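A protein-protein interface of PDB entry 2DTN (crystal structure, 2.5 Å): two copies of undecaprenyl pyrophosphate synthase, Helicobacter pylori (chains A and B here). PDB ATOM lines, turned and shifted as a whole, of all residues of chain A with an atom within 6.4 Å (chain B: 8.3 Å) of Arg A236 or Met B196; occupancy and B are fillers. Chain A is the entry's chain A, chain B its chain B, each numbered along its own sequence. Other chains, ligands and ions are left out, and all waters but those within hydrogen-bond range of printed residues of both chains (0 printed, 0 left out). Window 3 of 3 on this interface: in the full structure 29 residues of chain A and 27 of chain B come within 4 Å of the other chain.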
ATOM      1  N   MET A 196       4.590   1.669  25.099  1.00  0.00           N
ATOM      2  CA  MET A 196       4.658   0.316  25.625  1.00  0.00           C
ATOM      3  C   MET A 196       5.388   0.248  26.962  1.00  0.00           C
ATOM      4  O   MET A 196       6.408  -0.422  27.090  1.00  0.00           O
ATOM      5  CB  MET A 196       5.290  -0.632  24.593  1.00  0.00           C
ATOM      6  CG  MET A 196       4.309  -1.005  23.483  1.00  0.00           C
ATOM      7  SD  MET A 196       4.778  -2.384  22.373  1.00  0.00           S
ATOM      8  CE  MET A 196       5.338  -3.603  23.536  1.00  0.00           C
ATOM      9  N   ALA A 209      -1.285 -10.523  34.216  1.00  0.00           N
ATOM     10  CA  ALA A 209      -2.264  -9.989  33.283  1.00  0.00           C
ATOM     11  C   ALA A 209      -1.795 -10.054  31.845  1.00  0.00           C
ATOM     12  O   ALA A 209      -0.608  -9.898  31.552  1.00  0.00           O
ATOM     13  CB  ALA A 209      -2.577  -8.545  33.641  1.00  0.00           C
ATOM     14  N   GLU A 210      -2.741 -10.289  30.946  1.00  0.00           N
ATOM     15  CA  GLU A 210      -2.442 -10.321  29.525  1.00  0.00           C
ATOM     16  C   GLU A 210      -2.274  -8.861  29.142  1.00  0.00           C
ATOM     17  O   GLU A 210      -3.112  -8.024  29.484  1.00  0.00           O
ATOM     18  CB  GLU A 210      -3.604 -10.944  28.748  1.00  0.00           C
ATOM     19  CG  GLU A 210      -3.644 -12.453  28.824  1.00  0.00           C
ATOM     20  CD  GLU A 210      -2.411 -13.083  28.207  1.00  0.00           C
ATOM     21  OE1 GLU A 210      -1.921 -14.084  28.768  1.00  0.00           O
ATOM     22  OE2 GLU A 210      -1.935 -12.576  27.161  1.00  0.00           O
ATOM     23  N   LEU A 211      -1.191  -8.549  28.443  1.00  0.00           N
ATOM     24  CA  LEU A 211      -0.933  -7.174  28.051  1.00  0.00           C
ATOM     25  C   LEU A 211      -1.275  -6.898  26.598  1.00  0.00           C
ATOM     26  O   LEU A 211      -0.947  -7.672  25.710  1.00  0.00           O
ATOM     27  CB  LEU A 211       0.529  -6.826  28.313  1.00  0.00           C
ATOM     28  CG  LEU A 211       1.007  -7.241  29.704  1.00  0.00           C
ATOM     29  CD1 LEU A 211       2.500  -6.995  29.826  1.00  0.00           C
ATOM     30  CD2 LEU A 211       0.224  -6.483  30.765  1.00  0.00           C
ATOM     31  N   PHE A 212      -1.955  -5.786  26.373  1.00  0.00           N
ATOM     32  CA  PHE A 212      -2.337  -5.377  25.033  1.00  0.00           C
ATOM     33  C   PHE A 212      -1.952  -3.932  24.868  1.00  0.00           C
ATOM     34  O   PHE A 212      -1.984  -3.155  25.815  1.00  0.00           O
ATOM     35  CB  PHE A 212      -3.845  -5.512  24.801  1.00  0.00           C
ATOM     36  CG  PHE A 212      -4.307  -6.920  24.593  1.00  0.00           C
ATOM     37  CD1 PHE A 212      -4.408  -7.802  25.663  1.00  0.00           C
ATOM     38  CD2 PHE A 212      -4.661  -7.360  23.323  1.00  0.00           C
ATOM     39  CE1 PHE A 212      -4.862  -9.107  25.475  1.00  0.00           C
ATOM     40  CE2 PHE A 212      -5.117  -8.669  23.119  1.00  0.00           C
ATOM     41  CZ  PHE A 212      -5.220  -9.542  24.196  1.00  0.00           C
ATOM     42  N   PHE A 213      -1.588  -3.577  23.651  1.00  0.00           N
ATOM     43  CA  PHE A 213      -1.191  -2.219  23.347  1.00  0.00           C
ATOM     44  C   PHE A 213      -1.801  -1.905  22.006  1.00  0.00           C
ATOM     45  O   PHE A 213      -1.956  -2.793  21.167  1.00  0.00           O
ATOM     46  CB  PHE A 213       0.323  -2.129  23.265  1.00  0.00           C
ATOM     47  CG  PHE A 213       1.011  -2.564  24.508  1.00  0.00           C
ATOM     48  CD1 PHE A 213       1.288  -1.648  25.524  1.00  0.00           C
ATOM     49  CD2 PHE A 213       1.386  -3.898  24.677  1.00  0.00           C
ATOM     50  CE1 PHE A 213       1.936  -2.051  26.696  1.00  0.00           C
ATOM     51  CE2 PHE A 213       2.034  -4.315  25.842  1.00  0.00           C
ATOM     52  CZ  PHE A 213       2.311  -3.389  26.855  1.00  0.00           C
ATOM     53  N   SER A 231     -11.632 -10.234  21.922  1.00  0.00           N
ATOM     54  CA  SER A 231     -11.671 -11.426  21.095  1.00  0.00           C
ATOM     55  C   SER A 231     -10.258 -12.021  21.086  1.00  0.00           C
ATOM     56  O   SER A 231     -10.081 -13.209  21.343  1.00  0.00           O
ATOM     57  CB  SER A 231     -12.121 -11.079  19.671  1.00  0.00           C
ATOM     58  OG  SER A 231     -12.116 -12.234  18.849  1.00  0.00           O
ATOM     59  N   ASP A 232      -9.249 -11.196  20.806  1.00  0.00           N
ATOM     60  CA  ASP A 232      -7.871 -11.689  20.801  1.00  0.00           C
ATOM     61  C   ASP A 232      -7.472 -12.235  22.175  1.00  0.00           C
ATOM     62  O   ASP A 232      -6.717 -13.202  22.270  1.00  0.00           O
ATOM     63  CB  ASP A 232      -6.887 -10.595  20.388  1.00  0.00           C
ATOM     64  CG  ASP A 232      -7.074 -10.148  18.950  1.00  0.00           C
ATOM     65  OD1 ASP A 232      -7.539 -10.967  18.129  1.00  0.00           O
ATOM     66  OD2 ASP A 232      -6.738  -8.986  18.634  1.00  0.00           O
ATOM     67  N   PHE A 233      -7.978 -11.624  23.240  1.00  0.00           N
ATOM     68  CA  PHE A 233      -7.662 -12.097  24.582  1.00  0.00           C
ATOM     69  C   PHE A 233      -7.952 -13.596  24.681  1.00  0.00           C
ATOM     70  O   PHE A 233      -7.087 -14.376  25.064  1.00  0.00           O
ATOM     71  CB  PHE A 233      -8.483 -11.332  25.619  1.00  0.00           C
ATOM     72  CG  PHE A 233      -8.330 -11.849  27.020  1.00  0.00           C
ATOM     73  CD1 PHE A 233      -7.154 -11.642  27.731  1.00  0.00           C
ATOM     74  CD2 PHE A 233      -9.366 -12.551  27.634  1.00  0.00           C
ATOM     75  CE1 PHE A 233      -7.011 -12.125  29.033  1.00  0.00           C
ATOM     76  CE2 PHE A 233      -9.230 -13.039  28.937  1.00  0.00           C
ATOM     77  CZ  PHE A 233      -8.049 -12.825  29.636  1.00  0.00           C
ATOM     78  N   TYR A 234      -9.165 -14.002  24.320  1.00  0.00           N
ATOM     79  CA  TYR A 234      -9.527 -15.416  24.370  1.00  0.00           C
ATOM     80  C   TYR A 234      -8.642 -16.266  23.464  1.00  0.00           C
ATOM     81  O   TYR A 234      -8.253 -17.373  23.836  1.00  0.00           O
ATOM     82  CB  TYR A 234     -11.003 -15.602  24.003  1.00  0.00           C
ATOM     83  CG  TYR A 234     -11.940 -15.042  25.050  1.00  0.00           C
ATOM     84  CD1 TYR A 234     -12.799 -13.987  24.753  1.00  0.00           C
ATOM     85  CD2 TYR A 234     -11.939 -15.542  26.353  1.00  0.00           C
ATOM     86  CE1 TYR A 234     -13.632 -13.433  25.726  1.00  0.00           C
ATOM     87  CE2 TYR A 234     -12.770 -14.995  27.337  1.00  0.00           C
ATOM     88  CZ  TYR A 234     -13.611 -13.938  27.013  1.00  0.00           C
ATOM     89  OH  TYR A 234     -14.418 -13.374  27.979  1.00  0.00           O
ATOM     90  N   LYS A 235      -8.321 -15.761  22.278  1.00  0.00           N
ATOM     91  CA  LYS A 235      -7.456 -16.517  21.382  1.00  0.00           C
ATOM     92  C   LYS A 235      -6.145 -16.840  22.095  1.00  0.00           C
ATOM     93  O   LYS A 235      -5.639 -17.962  22.014  1.00  0.00           O
ATOM     94  CB  LYS A 235      -7.166 -15.724  20.113  1.00  0.00           C
ATOM     95  CG  LYS A 235      -8.375 -15.543  19.219  1.00  0.00           C
ATOM     96  CD  LYS A 235      -7.983 -14.924  17.892  1.00  0.00           C
ATOM     97  CE  LYS A 235      -9.163 -14.870  16.937  1.00  0.00           C
ATOM     98  NZ  LYS A 235      -8.752 -14.421  15.571  1.00  0.00           N
ATOM     99  N   ARG A 236      -5.600 -15.852  22.802  1.00  0.00           N
ATOM    100  CA  ARG A 236      -4.356 -16.052  23.536  1.00  0.00           C
ATOM    101  C   ARG A 236      -4.561 -17.148  24.570  1.00  0.00           C
ATOM    102  O   ARG A 236      -3.667 -17.956  24.819  1.00  0.00           O
ATOM    103  CB  ARG A 236      -3.931 -14.775  24.262  1.00  0.00           C
ATOM    104  CG  ARG A 236      -3.539 -13.614  23.381  1.00  0.00           C
ATOM    105  CD  ARG A 236      -2.843 -12.569  24.238  1.00  0.00           C
ATOM    106  NE  ARG A 236      -2.538 -11.328  23.530  1.00  0.00           N
ATOM    107  CZ  ARG A 236      -1.968 -10.274  24.109  1.00  0.00           C
ATOM    108  NH1 ARG A 236      -1.644 -10.323  25.394  1.00  0.00           N
ATOM    109  NH2 ARG A 236      -1.732  -9.170  23.415  1.00  0.00           N
ATOM    110  N   VAL A 237      -5.744 -17.162  25.176  1.00  0.00           N
ATOM    111  CA  VAL A 237      -6.071 -18.152  26.189  1.00  0.00           C
ATOM    112  C   VAL A 237      -6.628 -19.426  25.539  1.00  0.00           C
ATOM    113  O   VAL A 237      -7.708 -19.895  25.962  1.00  0.00           O
ATOM    114  CB  VAL A 237      -7.107 -17.584  27.194  1.00  0.00           C
ATOM    115  CG1 VAL A 237      -7.294 -18.544  28.373  1.00  0.00           C
ATOM    116  CG2 VAL A 237      -6.657 -16.218  27.678  1.00  0.00           C
ATOM    117  N   ILE B  22      12.992 -12.294  29.857  1.00  0.00           N
ATOM    118  CA  ILE B  22      12.299 -13.492  30.280  1.00  0.00           C
ATOM    119  C   ILE B  22      12.589 -14.507  29.159  1.00  0.00           C
ATOM    120  O   ILE B  22      12.168 -14.323  28.014  1.00  0.00           O
ATOM    121  CB  ILE B  22      10.803 -13.237  30.406  1.00  0.00           C
ATOM    122  CG1 ILE B  22      10.570 -12.104  31.412  1.00  0.00           C
ATOM    123  CG2 ILE B  22      10.091 -14.524  30.791  1.00  0.00           C
ATOM    124  CD1 ILE B  22       9.115 -11.718  31.616  1.00  0.00           C
ATOM    125  N   ASP B  24      11.875 -17.674  27.479  1.00  0.00           N
ATOM    126  CA  ASP B  24      10.727 -18.554  27.373  1.00  0.00           C
ATOM    127  C   ASP B  24      10.713 -19.205  25.986  1.00  0.00           C
ATOM    128  O   ASP B  24      11.311 -18.692  25.046  1.00  0.00           O
ATOM    129  CB  ASP B  24       9.475 -17.703  27.596  1.00  0.00           C
ATOM    130  CG  ASP B  24       8.207 -18.523  27.714  1.00  0.00           C
ATOM    131  OD1 ASP B  24       8.299 -19.756  27.871  1.00  0.00           O
ATOM    132  OD2 ASP B  24       7.110 -17.924  27.661  1.00  0.00           O
ATOM    133  N   ARG B 191      10.504  -9.951  26.514  1.00  0.00           N
ATOM    134  CA  ARG B 191      10.037 -11.303  26.721  1.00  0.00           C
ATOM    135  C   ARG B 191      10.050 -12.077  25.401  1.00  0.00           C
ATOM    136  O   ARG B 191       9.420 -11.663  24.428  1.00  0.00           O
ATOM    137  CB  ARG B 191       8.629 -11.328  27.318  1.00  0.00           C
ATOM    138  CG  ARG B 191       8.059 -12.747  27.353  1.00  0.00           C
ATOM    139  CD  ARG B 191       6.869 -12.903  28.267  1.00  0.00           C
ATOM    140  NE  ARG B 191       6.557 -14.320  28.429  1.00  0.00           N
ATOM    141  CZ  ARG B 191       5.937 -14.838  29.482  1.00  0.00           C
ATOM    142  NH1 ARG B 191       5.553 -14.057  30.482  1.00  0.00           N
ATOM    143  NH2 ARG B 191       5.722 -16.140  29.547  1.00  0.00           N
ATOM    144  N   THR B 192      10.788 -13.186  25.368  1.00  0.00           N
ATOM    145  CA  THR B 192      10.863 -14.013  24.167  1.00  0.00           C
ATOM    146  C   THR B 192       9.775 -15.064  24.325  1.00  0.00           C
ATOM    147  O   THR B 192       9.136 -15.131  25.373  1.00  0.00           O
ATOM    148  CB  THR B 192      12.246 -14.725  24.031  1.00  0.00           C
ATOM    149  OG1 THR B 192      12.514 -15.484  25.216  1.00  0.00           O
ATOM    150  CG2 THR B 192      13.385 -13.698  23.815  1.00  0.00           C
ATOM    151  N   GLY B 193       9.546 -15.873  23.296  1.00  0.00           N
ATOM    152  CA  GLY B 193       8.533 -16.909  23.409  1.00  0.00           C
ATOM    153  C   GLY B 193       7.156 -16.621  22.833  1.00  0.00           C
ATOM    154  O   GLY B 193       6.417 -17.558  22.560  1.00  0.00           O
ATOM    155  N   GLY B 194       6.789 -15.352  22.668  1.00  0.00           N
ATOM    156  CA  GLY B 194       5.493 -15.035  22.097  1.00  0.00           C
ATOM    157  C   GLY B 194       4.438 -14.559  23.071  1.00  0.00           C
ATOM    158  O   GLY B 194       3.545 -13.803  22.697  1.00  0.00           O
ATOM    159  N   GLU B 195       4.529 -14.994  24.323  1.00  0.00           N
ATOM    160  CA  GLU B 195       3.557 -14.597  25.334  1.00  0.00           C
ATOM    161  C   GLU B 195       3.723 -13.128  25.696  1.00  0.00           C
ATOM    162  O   GLU B 195       4.810 -12.573  25.594  1.00  0.00           O
ATOM    163  CB  GLU B 195       3.710 -15.454  26.593  1.00  0.00           C
ATOM    164  CG  GLU B 195       3.607 -16.947  26.353  1.00  0.00           C
ATOM    165  CD  GLU B 195       2.299 -17.349  25.711  1.00  0.00           C
ATOM    166  OE1 GLU B 195       2.104 -18.560  25.455  1.00  0.00           O
ATOM    167  OE2 GLU B 195       1.463 -16.454  25.458  1.00  0.00           O
ATOM    168  N   MET B 196       2.638 -12.505  26.132  1.00  0.00           N
ATOM    169  CA  MET B 196       2.671 -11.101  26.484  1.00  0.00           C
ATOM    170  C   MET B 196       2.120 -10.838  27.878  1.00  0.00           C
ATOM    171  O   MET B 196       0.963 -10.478  28.050  1.00  0.00           O
ATOM    172  CB  MET B 196       1.903 -10.300  25.426  1.00  0.00           C
ATOM    173  CG  MET B 196       2.539 -10.380  24.046  1.00  0.00           C
ATOM    174  SD  MET B 196       1.679  -9.443  22.778  1.00  0.00           S
ATOM    175  CE  MET B 196       2.287  -7.751  23.083  1.00  0.00           C
ATOM    176  N   ARG B 197       2.981 -11.040  28.864  1.00  0.00           N
ATOM    177  CA  ARG B 197       2.690 -10.843  30.279  1.00  0.00           C
ATOM    178  C   ARG B 197       4.029 -10.859  31.002  1.00  0.00           C
ATOM    179  O   ARG B 197       4.988 -11.442  30.521  1.00  0.00           O
ATOM    180  CB  ARG B 197       1.756 -11.938  30.830  1.00  0.00           C
ATOM    181  CG  ARG B 197       1.894 -13.310  30.196  1.00  0.00           C
ATOM    182  CD  ARG B 197       0.710 -14.206  30.584  1.00  0.00           C
ATOM    183  NE  ARG B 197       0.435 -15.198  29.548  1.00  0.00           N
ATOM    184  CZ  ARG B 197       1.126 -16.319  29.372  1.00  0.00           C
ATOM    185  NH1 ARG B 197       2.138 -16.613  30.177  1.00  0.00           N
ATOM    186  NH2 ARG B 197       0.824 -17.133  28.372  1.00  0.00           N
ATOM    187  N   LEU B 198       4.092 -10.214  32.154  1.00  0.00           N
ATOM    188  CA  LEU B 198       5.334 -10.111  32.902  1.00  0.00           C
ATOM    189  C   LEU B 198       5.644 -11.331  33.747  1.00  0.00           C
ATOM    190  O   LEU B 198       6.790 -11.554  34.125  1.00  0.00           O
ATOM    191  CB  LEU B 198       5.282  -8.866  33.783  1.00  0.00           C
ATOM    192  CG  LEU B 198       4.685  -7.633  33.091  1.00  0.00           C
ATOM    193  CD1 LEU B 198       4.588  -6.494  34.088  1.00  0.00           C
ATOM    194  CD2 LEU B 198       5.528  -7.233  31.903  1.00  0.00           C
ATOM    195  N   SER B 199       4.623 -12.118  34.041  1.00  0.00           N
ATOM    196  CA  SER B 199       4.794 -13.325  34.834  1.00  0.00           C
ATOM    197  C   SER B 199       5.545 -13.173  36.150  1.00  0.00           C
ATOM    198  O   SER B 199       6.487 -13.914  36.411  1.00  0.00           O
ATOM    199  CB  SER B 199       5.458 -14.428  33.998  1.00  0.00           C
ATOM    200  OG  SER B 199       4.558 -14.936  33.018  1.00  0.00           O
ATOM    201  N   LEU B 211       8.690  -1.960  27.226  1.00  0.00           N
ATOM    202  CA  LEU B 211       8.394  -3.372  27.051  1.00  0.00           C
ATOM    203  C   LEU B 211       8.599  -3.846  25.619  1.00  0.00           C
ATOM    204  O   LEU B 211       8.295  -3.135  24.665  1.00  0.00           O
ATOM    205  CB  LEU B 211       6.960  -3.650  27.483  1.00  0.00           C
ATOM    206  CG  LEU B 211       6.666  -3.248  28.936  1.00  0.00           C
ATOM    207  CD1 LEU B 211       5.156  -3.245  29.177  1.00  0.00           C
ATOM    208  CD2 LEU B 211       7.362  -4.198  29.905  1.00  0.00           C
ATOM    209  N   PHE B 212       9.125  -5.054  25.474  1.00  0.00           N
ATOM    210  CA  PHE B 212       9.337  -5.630  24.160  1.00  0.00           C
ATOM    211  C   PHE B 212       8.965  -7.086  24.217  1.00  0.00           C
ATOM    212  O   PHE B 212       9.262  -7.778  25.186  1.00  0.00           O
ATOM    213  CB  PHE B 212      10.789  -5.513  23.708  1.00  0.00           C
ATOM    214  CG  PHE B 212      11.151  -4.162  23.166  1.00  0.00           C
ATOM    215  CD1 PHE B 212      11.343  -3.080  24.022  1.00  0.00           C
ATOM    216  CD2 PHE B 212      11.319  -3.972  21.800  1.00  0.00           C
ATOM    217  CE1 PHE B 212      11.700  -1.831  23.527  1.00  0.00           C
ATOM    218  CE2 PHE B 212      11.677  -2.717  21.300  1.00  0.00           C
ATOM    219  CZ  PHE B 212      11.868  -1.650  22.169  1.00  0.00           C
ATOM    220  N   PHE B 213       8.316  -7.543  23.158  1.00  0.00           N
ATOM    221  CA  PHE B 213       7.880  -8.917  23.047  1.00  0.00           C
ATOM    222  C   PHE B 213       8.310  -9.422  21.695  1.00  0.00           C
ATOM    223  O   PHE B 213       8.195  -8.710  20.696  1.00  0.00           O
ATOM    224  CB  PHE B 213       6.365  -8.972  23.156  1.00  0.00           C
ATOM    225  CG  PHE B 213       5.848  -8.349  24.410  1.00  0.00           C
ATOM    226  CD1 PHE B 213       5.872  -9.053  25.608  1.00  0.00           C
ATOM    227  CD2 PHE B 213       5.421  -7.020  24.416  1.00  0.00           C
ATOM    228  CE1 PHE B 213       5.482  -8.438  26.792  1.00  0.00           C
ATOM    229  CE2 PHE B 213       5.032  -6.408  25.599  1.00  0.00           C
ATOM    230  CZ  PHE B 213       5.064  -7.112  26.783  1.00  0.00           C
ATOM    231  N   THR B 214       8.834 -10.639  21.669  1.00  0.00           N
ATOM    232  CA  THR B 214       9.240 -11.240  20.421  1.00  0.00           C
ATOM    233  C   THR B 214       8.714 -12.676  20.377  1.00  0.00           C
ATOM    234  O   THR B 214       8.755 -13.393  21.380  1.00  0.00           O
ATOM    235  CB  THR B 214      10.782 -11.211  20.263  1.00  0.00           C
ATOM    236  OG1 THR B 214      11.136 -11.778  19.001  1.00  0.00           O
ATOM    237  CG2 THR B 214      11.466 -11.981  21.369  1.00  0.00           C
ATOM    238  N   PRO B 215       8.166 -13.097  19.225  1.00  0.00           N
ATOM    239  CA  PRO B 215       7.631 -14.457  19.061  1.00  0.00           C
ATOM    240  C   PRO B 215       8.753 -15.488  19.015  1.00  0.00           C
ATOM    241  O   PRO B 215       8.513 -16.681  19.143  1.00  0.00           O
ATOM    242  CB  PRO B 215       6.900 -14.398  17.719  1.00  0.00           C
ATOM    243  CG  PRO B 215       6.540 -12.951  17.571  1.00  0.00           C
ATOM    244  CD  PRO B 215       7.777 -12.242  18.096  1.00  0.00           C
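NH1 of Arg A236 is in salt-bridge range of OE2 of Glu A210 (2.9 Å).
O of Leu A211 lies within hydrogen-bond range of NH1 of Arg A236 (2.8 Å).
NH1 of Arg B191 sits at hydrogen-bond distance from O of Arg B197 (2.7 Å).
NH2 of Arg B197 is in salt-bridge range of OE2 of Glu B195 (3.1 Å).
Arg A236 touches just one residue of chain B: Met B196.
Met B196 touches just these residues of chain A: Ala A209, Glu A210, Leu A211 and Arg A236.
Of the printed residues of chain B, Leu A211 touches Met B196 (2.9 Å), Arg B197 (3.9 Å), Leu B198 (3.7 Å) and Phe B213 (3.98 Å).
Printed residues of chain B within 4 Å of Phe A213: Leu B211 (3.7 Å) and Phe B213 (3.7 Å).
Printed residues of chain B within 4 Å of Met A196: Leu B211 and Phe B213.
Of the printed residues of chain A, Leu B211 touches Met A196 and Phe A213.
Among the printed residues, merely in contact across the chains: Ala A209 with Arg B197 (3.2 Å), Met A196 with Phe B213 (3.5 Å), Phe A213 with Phe B213 (3.7 Å), Phe A213 with Leu B211 (3.7 Å), Leu A211 with Leu B198 (3.7 Å), Glu A210 with Met B196 (3.7 Å), Leu A211 with Arg B197 (3.9 Å), Ala A209 with Met B196 (3.9 Å) and Leu A211 with Phe B213 (3.98 Å).
Of the 13 printed residues of chain A, 6 touch a printed residue of chain B.
Printed residues of chain A that touch a printed residue of chain B: Met A196, Ala A209, Glu A210, Leu A211, Phe A213 and Arg A236.
Hydrophobic or aromatic side chains of chain A that line the printed part of chain B: Met A196, Leu A211 and Phe A213.
Printed residues of chain B that touch a printed residue of chain A: Met B196, Arg B197, Leu B198, Leu B211 and Phe B213.
Hydrophobic or aromatic side chains of chain B within 4 Å of the printed part of chain A: Met B196, Leu B198, Leu B211 and Phe B213.
Among the printed residues, Asp or Glu carboxylates within 4 Å of a Lys or Arg side-chain nitrogen of the other chain: Glu A210 with Arg B197 (2.7 Å).
The backbone carbonyl oxygen of Met A196 lies within hydrogen-bond range of the backbone NH of Leu B211 (2.8 Å).
The side-chain carboxylate (OE1) of Glu A210 lies within salt-bridge range of the guanidinium group (NE) of Arg B197.
The backbone NH (N) of Leu A211 sits at hydrogen-bond distance from the backbone carbonyl oxygen (O) of Met B196.
The side-chain sulfur of Met B196 sits at hydrogen-bond distance from the guanidinium group of Arg A236 (3.5 Å).
Met A196 touches Leu B211, and with the chains exchanged Leu A211 touches Met B196.
Met A196 touches Phe B213, but with the chains exchanged Phe A213 does not touch Met B196 (4.3 Å).
Leu A211 touches Phe B213, and with the chains exchanged Phe A213 touches Leu B211.
Phe A213 touches its own counterpart, Phe B213.
4 positions are printed for both chains.
Of the 13 pairs that touch across the chains among the printed residues, 5 have their exchanged pair printed and touching as well.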
